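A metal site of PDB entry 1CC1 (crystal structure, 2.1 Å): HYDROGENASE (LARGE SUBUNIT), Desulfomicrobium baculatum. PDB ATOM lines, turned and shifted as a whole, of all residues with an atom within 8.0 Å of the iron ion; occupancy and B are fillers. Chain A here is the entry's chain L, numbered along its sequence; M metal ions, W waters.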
ATOM      1  N   PHE A  47      15.453 -16.906  -7.417  1.00  0.00           N
ATOM      2  CA  PHE A  47      14.514 -17.934  -7.037  1.00  0.00           C
ATOM      3  C   PHE A  47      13.328 -17.326  -6.308  1.00  0.00           C
ATOM      4  O   PHE A  47      13.470 -16.330  -5.581  1.00  0.00           O
ATOM      5  CB  PHE A  47      15.236 -19.002  -6.195  1.00  0.00           C
ATOM      6  CG  PHE A  47      14.332 -19.997  -5.525  1.00  0.00           C
ATOM      7  CD1 PHE A  47      13.897 -21.137  -6.199  1.00  0.00           C
ATOM      8  CD2 PHE A  47      13.971 -19.830  -4.197  1.00  0.00           C
ATOM      9  CE1 PHE A  47      13.123 -22.101  -5.542  1.00  0.00           C
ATOM     10  CE2 PHE A  47      13.189 -20.776  -3.529  1.00  0.00           C
ATOM     11  CZ  PHE A  47      12.764 -21.916  -4.204  1.00  0.00           C
ATOM     12  N   GLU A  51       6.592 -23.746  -6.175  1.00  0.00           N
ATOM     13  CA  GLU A  51       6.253 -25.069  -5.697  1.00  0.00           C
ATOM     14  C   GLU A  51       6.041 -25.107  -4.182  1.00  0.00           C
ATOM     15  O   GLU A  51       5.400 -26.013  -3.650  1.00  0.00           O
ATOM     16  CB  GLU A  51       7.328 -26.064  -6.142  1.00  0.00           C
ATOM     17  CG  GLU A  51       7.383 -26.208  -7.656  1.00  0.00           C
ATOM     18  CD  GLU A  51       8.751 -26.628  -8.190  1.00  0.00           C
ATOM     19  OE1 GLU A  51       8.793 -27.227  -9.291  1.00  0.00           O
ATOM     20  OE2 GLU A  51       9.757 -26.334  -7.537  1.00  0.00           O
ATOM     21  N   GLU A 285      14.761 -35.207 -12.188  1.00  0.00           N
ATOM     22  CA  GLU A 285      15.522 -33.999 -11.976  1.00  0.00           C
ATOM     23  C   GLU A 285      16.617 -34.259 -10.972  1.00  0.00           C
ATOM     24  O   GLU A 285      16.411 -34.949  -9.980  1.00  0.00           O
ATOM     25  CB  GLU A 285      14.648 -32.866 -11.478  1.00  0.00           C
ATOM     26  CG  GLU A 285      13.651 -32.345 -12.492  1.00  0.00           C
ATOM     27  CD  GLU A 285      12.893 -31.160 -11.938  1.00  0.00           C
ATOM     28  OE1 GLU A 285      13.147 -30.023 -12.399  1.00  0.00           O
ATOM     29  OE2 GLU A 285      12.076 -31.372 -11.021  1.00  0.00           O
ATOM     30  N   PHE A 292      19.543 -26.882  -4.024  1.00  0.00           N
ATOM     31  CA  PHE A 292      18.399 -27.595  -3.457  1.00  0.00           C
ATOM     32  C   PHE A 292      18.859 -28.870  -2.806  1.00  0.00           C
ATOM     33  O   PHE A 292      19.838 -29.468  -3.231  1.00  0.00           O
ATOM     34  CB  PHE A 292      17.394 -27.984  -4.563  1.00  0.00           C
ATOM     35  CG  PHE A 292      16.722 -26.819  -5.192  1.00  0.00           C
ATOM     36  CD1 PHE A 292      17.186 -26.296  -6.396  1.00  0.00           C
ATOM     37  CD2 PHE A 292      15.605 -26.236  -4.596  1.00  0.00           C
ATOM     38  CE1 PHE A 292      16.563 -25.214  -7.007  1.00  0.00           C
ATOM     39  CE2 PHE A 292      14.963 -25.149  -5.191  1.00  0.00           C
ATOM     40  CZ  PHE A 292      15.457 -24.636  -6.402  1.00  0.00           C
ATOM     41  N   TYR A 302       9.314 -36.305 -11.288  1.00  0.00           N
ATOM     42  CA  TYR A 302       8.518 -35.137 -10.947  1.00  0.00           C
ATOM     43  C   TYR A 302       7.319 -35.384 -10.016  1.00  0.00           C
ATOM     44  O   TYR A 302       6.982 -34.507  -9.211  1.00  0.00           O
ATOM     45  CB  TYR A 302       8.080 -34.420 -12.230  1.00  0.00           C
ATOM     46  CG  TYR A 302       7.224 -35.247 -13.163  1.00  0.00           C
ATOM     47  CD1 TYR A 302       5.852 -35.393 -12.932  1.00  0.00           C
ATOM     48  CD2 TYR A 302       7.775 -35.855 -14.300  1.00  0.00           C
ATOM     49  CE1 TYR A 302       5.047 -36.103 -13.793  1.00  0.00           C
ATOM     50  CE2 TYR A 302       6.967 -36.578 -15.179  1.00  0.00           C
ATOM     51  CZ  TYR A 302       5.619 -36.694 -14.922  1.00  0.00           C
ATOM     52  OH  TYR A 302       4.814 -37.396 -15.778  1.00  0.00           O
ATOM     53  N   GLY A 305       8.850 -35.039  -6.825  1.00  0.00           N
ATOM     54  CA  GLY A 305       9.800 -33.950  -6.714  1.00  0.00           C
ATOM     55  C   GLY A 305       9.700 -33.174  -5.407  1.00  0.00           C
ATOM     56  O   GLY A 305       8.649 -33.088  -4.769  1.00  0.00           O
ATOM     57  N   GLU A 306      10.835 -32.601  -5.009  1.00  0.00           N
ATOM     58  CA  GLU A 306      10.940 -31.825  -3.772  1.00  0.00           C
ATOM     59  C   GLU A 306      11.558 -30.467  -4.041  1.00  0.00           C
ATOM     60  O   GLU A 306      12.504 -30.338  -4.828  1.00  0.00           O
ATOM     61  CB  GLU A 306      11.809 -32.543  -2.757  1.00  0.00           C
ATOM     62  CG  GLU A 306      11.333 -33.920  -2.347  1.00  0.00           C
ATOM     63  CD  GLU A 306      12.450 -34.772  -1.810  1.00  0.00           C
ATOM     64  OE1 GLU A 306      13.536 -34.229  -1.518  1.00  0.00           O
ATOM     65  OE2 GLU A 306      12.246 -35.996  -1.698  1.00  0.00           O
ATOM     66  N   THR A 307      11.079 -29.470  -3.311  1.00  0.00           N
ATOM     67  CA  THR A 307      11.586 -28.118  -3.450  1.00  0.00           C
ATOM     68  C   THR A 307      12.035 -27.548  -2.096  1.00  0.00           C
ATOM     69  O   THR A 307      11.282 -26.881  -1.371  1.00  0.00           O
ATOM     70  CB  THR A 307      10.538 -27.204  -4.151  1.00  0.00           C
ATOM     71  OG1 THR A 307      10.196 -27.768  -5.428  1.00  0.00           O
ATOM     72  CG2 THR A 307      11.112 -25.807  -4.361  1.00  0.00           C
ATOM     73  N   PHE A 319      20.109 -21.962  -9.391  1.00  0.00           N
ATOM     74  CA  PHE A 319      18.796 -22.283  -8.848  1.00  0.00           C
ATOM     75  C   PHE A 319      18.007 -23.124  -9.828  1.00  0.00           C
ATOM     76  O   PHE A 319      16.841 -23.443  -9.580  1.00  0.00           O
ATOM     77  CB  PHE A 319      17.980 -21.037  -8.543  1.00  0.00           C
ATOM     78  CG  PHE A 319      18.365 -20.385  -7.266  1.00  0.00           C
ATOM     79  CD1 PHE A 319      18.960 -19.136  -7.273  1.00  0.00           C
ATOM     80  CD2 PHE A 319      18.189 -21.045  -6.041  1.00  0.00           C
ATOM     81  CE1 PHE A 319      19.386 -18.535  -6.096  1.00  0.00           C
ATOM     82  CE2 PHE A 319      18.605 -20.449  -4.854  1.00  0.00           C
ATOM     83  CZ  PHE A 319      19.198 -19.198  -4.883  1.00  0.00           C
ATOM     84  N   LYS A 321      17.329 -26.573 -11.551  1.00  0.00           N
ATOM     85  CA  LYS A 321      17.520 -28.005 -11.303  1.00  0.00           C
ATOM     86  C   LYS A 321      17.954 -28.591 -12.651  1.00  0.00           C
ATOM     87  O   LYS A 321      17.918 -27.891 -13.669  1.00  0.00           O
ATOM     88  CB  LYS A 321      16.220 -28.669 -10.826  1.00  0.00           C
ATOM     89  CG  LYS A 321      15.681 -28.219  -9.467  1.00  0.00           C
ATOM     90  CD  LYS A 321      14.468 -29.044  -9.084  1.00  0.00           C
ATOM     91  CE  LYS A 321      13.967 -28.780  -7.682  1.00  0.00           C
ATOM     92  NZ  LYS A 321      12.566 -29.293  -7.527  1.00  0.00           N
ATOM     93  N   LEU A 429       5.784 -29.397 -18.168  1.00  0.00           N
ATOM     94  CA  LEU A 429       4.797 -30.202 -17.478  1.00  0.00           C
ATOM     95  C   LEU A 429       4.565 -29.671 -16.082  1.00  0.00           C
ATOM     96  O   LEU A 429       5.457 -29.065 -15.479  1.00  0.00           O
ATOM     97  CB  LEU A 429       5.170 -31.696 -17.436  1.00  0.00           C
ATOM     98  CG  LEU A 429       6.113 -32.214 -16.338  1.00  0.00           C
ATOM     99  CD1 LEU A 429       5.347 -32.643 -15.052  1.00  0.00           C
ATOM    100  CD2 LEU A 429       6.858 -33.374 -16.934  1.00  0.00           C
ATOM    101  N   TYR A 442       3.128 -29.569  -5.805  1.00  0.00           N
ATOM    102  CA  TYR A 442       3.000 -29.028  -7.146  1.00  0.00           C
ATOM    103  C   TYR A 442       4.394 -28.965  -7.688  1.00  0.00           C
ATOM    104  O   TYR A 442       5.256 -28.308  -7.112  1.00  0.00           O
ATOM    105  CB  TYR A 442       2.367 -27.630  -7.123  1.00  0.00           C
ATOM    106  CG  TYR A 442       1.694 -27.230  -8.441  1.00  0.00           C
ATOM    107  CD1 TYR A 442       0.307 -27.275  -8.576  1.00  0.00           C
ATOM    108  CD2 TYR A 442       2.455 -26.799  -9.541  1.00  0.00           C
ATOM    109  CE1 TYR A 442      -0.318 -26.900  -9.773  1.00  0.00           C
ATOM    110  CE2 TYR A 442       1.838 -26.423 -10.761  1.00  0.00           C
ATOM    111  CZ  TYR A 442       0.454 -26.479 -10.857  1.00  0.00           C
ATOM    112  OH  TYR A 442      -0.189 -26.113 -12.035  1.00  0.00           O
ATOM    113  N   GLN A 443       4.655 -29.722  -8.741  1.00  0.00           N
ATOM    114  CA  GLN A 443       5.972 -29.743  -9.348  1.00  0.00           C
ATOM    115  C   GLN A 443       5.952 -29.281 -10.809  1.00  0.00           C
ATOM    116  O   GLN A 443       5.112 -29.698 -11.596  1.00  0.00           O
ATOM    117  CB  GLN A 443       6.631 -31.118  -9.166  1.00  0.00           C
ATOM    118  CG  GLN A 443       7.036 -31.414  -7.729  1.00  0.00           C
ATOM    119  CD  GLN A 443       8.123 -30.477  -7.217  1.00  0.00           C
ATOM    120  OE1 GLN A 443       8.040 -29.940  -6.101  1.00  0.00           O
ATOM    121  NE2 GLN A 443       9.160 -30.287  -8.022  1.00  0.00           N
ATOM    122  N   ILE A 444       6.861 -28.362 -11.132  1.00  0.00           N
ATOM    123  CA  ILE A 444       6.967 -27.781 -12.454  1.00  0.00           C
ATOM    124  C   ILE A 444       8.294 -28.126 -13.160  1.00  0.00           C
ATOM    125  O   ILE A 444       9.377 -27.892 -12.638  1.00  0.00           O
ATOM    126  CB  ILE A 444       6.827 -26.230 -12.364  1.00  0.00           C
ATOM    127  CG1 ILE A 444       5.498 -25.857 -11.688  1.00  0.00           C
ATOM    128  CG2 ILE A 444       6.940 -25.584 -13.742  1.00  0.00           C
ATOM    129  CD1 ILE A 444       5.458 -24.447 -11.167  1.00  0.00           C
ATOM    130  N   VAL A 445       8.179 -28.738 -14.340  1.00  0.00           N
ATOM    131  CA  VAL A 445       9.348 -29.091 -15.133  1.00  0.00           C
ATOM    132  C   VAL A 445       9.144 -28.267 -16.416  1.00  0.00           C
ATOM    133  O   VAL A 445       8.453 -28.665 -17.362  1.00  0.00           O
ATOM    134  CB  VAL A 445       9.449 -30.605 -15.349  1.00  0.00           C
ATOM    135  CG1 VAL A 445      10.697 -30.965 -16.162  1.00  0.00           C
ATOM    136  CG2 VAL A 445       9.525 -31.271 -13.982  1.00  0.00           C
ATOM    137  N   SER A 446       9.778 -27.091 -16.398  1.00  0.00           N
ATOM    138  CA  SER A 446       9.592 -26.068 -17.422  1.00  0.00           C
ATOM    139  C   SER A 446      10.601 -25.573 -18.445  1.00  0.00           C
ATOM    140  O   SER A 446      11.459 -24.745 -18.118  1.00  0.00           O
ATOM    141  CB  SER A 446       9.079 -24.818 -16.709  1.00  0.00           C
ATOM    142  OG  SER A 446      10.187 -24.219 -16.043  1.00  0.00           O
ATOM    143  N   LEU A 449      14.303 -24.873 -18.269  1.00  0.00           N
ATOM    144  CA  LEU A 449      14.827 -25.744 -17.238  1.00  0.00           C
ATOM    145  C   LEU A 449      15.720 -26.799 -17.923  1.00  0.00           C
ATOM    146  O   LEU A 449      16.830 -27.059 -17.482  1.00  0.00           O
ATOM    147  CB  LEU A 449      13.679 -26.425 -16.481  1.00  0.00           C
ATOM    148  CG  LEU A 449      14.068 -27.557 -15.518  1.00  0.00           C
ATOM    149  CD1 LEU A 449      14.854 -27.010 -14.335  1.00  0.00           C
ATOM    150  CD2 LEU A 449      12.806 -28.275 -15.050  1.00  0.00           C
ATOM    151  N   CYS A 495      11.243 -18.966 -15.782  1.00  0.00           N
ATOM    152  CA  CYS A 495      10.659 -20.289 -15.976  1.00  0.00           C
ATOM    153  C   CYS A 495      11.562 -21.407 -15.506  1.00  0.00           C
ATOM    154  O   CYS A 495      11.120 -22.325 -14.855  1.00  0.00           O
ATOM    155  CB  CYS A 495      10.343 -20.528 -17.452  1.00  0.00           C
ATOM    156  SG  CYS A 495       8.831 -19.714 -18.009  1.00  0.00           S
ATOM    157  N   ALA A 496      12.842 -21.330 -15.850  1.00  0.00           N
ATOM    158  CA  ALA A 496      13.810 -22.331 -15.478  1.00  0.00           C
ATOM    159  C   ALA A 496      13.901 -22.577 -13.983  1.00  0.00           C
ATOM    160  O   ALA A 496      14.066 -23.720 -13.550  1.00  0.00           O
ATOM    161  CB  ALA A 496      15.165 -21.953 -16.026  1.00  0.00           C
ATOM    162  N   VAL A 497      13.811 -21.499 -13.185  1.00  0.00           N
ATOM    163  CA  VAL A 497      13.893 -21.608 -11.728  1.00  0.00           C
ATOM    164  C   VAL A 497      12.544 -21.653 -10.996  1.00  0.00           C
ATOM    165  O   VAL A 497      12.369 -22.458 -10.069  1.00  0.00           O
ATOM    166  CB  VAL A 497      14.677 -20.413 -11.101  1.00  0.00           C
ATOM    167  CG1 VAL A 497      14.693 -20.573  -9.564  1.00  0.00           C
ATOM    168  CG2 VAL A 497      16.068 -20.340 -11.682  1.00  0.00           C
ATOM    169  N   HIS A 498      11.621 -20.775 -11.380  1.00  0.00           N
ATOM    170  CA  HIS A 498      10.291 -20.620 -10.745  1.00  0.00           C
ATOM    171  C   HIS A 498      10.397 -20.523  -9.209  1.00  0.00           C
ATOM    172  O   HIS A 498       9.665 -21.253  -8.505  1.00  0.00           O
ATOM    173  CB  HIS A 498       9.223 -21.667 -11.226  1.00  0.00           C
ATOM    174  CG  HIS A 498       9.750 -23.053 -11.443  1.00  0.00           C
ATOM    175  ND1 HIS A 498      10.377 -23.448 -12.604  1.00  0.00           N
ATOM    176  CD2 HIS A 498       9.725 -24.154 -10.644  1.00  0.00           C
ATOM    177  CE1 HIS A 498      10.721 -24.709 -12.523  1.00  0.00           C
ATOM    178  NE2 HIS A 498      10.327 -25.166 -11.344  1.00  0.00           N
ATOM    179  OXT HIS A 498      11.265 -19.765  -8.715  1.00  0.00           O
HETATM  180 FE    FE M   1      10.530 -27.416 -10.714  1.00  0.00          FE
HETATM  181  O   HOH W   1      10.531 -29.598 -10.012  1.00  0.00           O
HETATM  182  O   HOH W   2      12.029 -26.813  -8.799  1.00  0.00           O
HETATM  183  O   HOH W   3      12.260 -27.661 -11.825  1.00  0.00           O
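The side-chain amide nitrogen (NE2) of Gln 443 sits close to the side-chain carboxylate (OE1) of Glu 51 (3.3 Å). The side-chain carboxylate (OE2) of Glu 51 sits at hydrogen-bond distance from the side-chain hydroxyl (OG1) of Thr 307 (2.6 Å). The backbone carbonyl oxygen (O) of Cys 495 is in hydrogen-bond range of a ring nitrogen (ND1) of His 498.
The nearest printed residue that does not touch the iron ion is Glu 285 (4.1 Å).
The iron ion is bound by water W3 (2.1 Å), the side-chain carboxylate of Glu 51 (2.3 Å), water W1 (2.3 Å), the backbone carbonyl oxygen of Ile 444 (2.3 Å), a ring nitrogen (NE2) of His 498 (2.3 Å) and water W2 (2.5 Å). The iron ion has six donor atoms within binding distance.
Water W1 lies within hydrogen-bond range of NE2 of Gln 443 (2.5 Å), OE2 of Glu 285 (2.6 Å) and NZ of Lys 321 (3.2 Å). Water W2 lies within hydrogen-bond range of the side-chain carboxylate (OE2) of Glu 51 (2.6 Å) and the side-chain amino group (NZ) of Lys 321 (2.8 Å).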
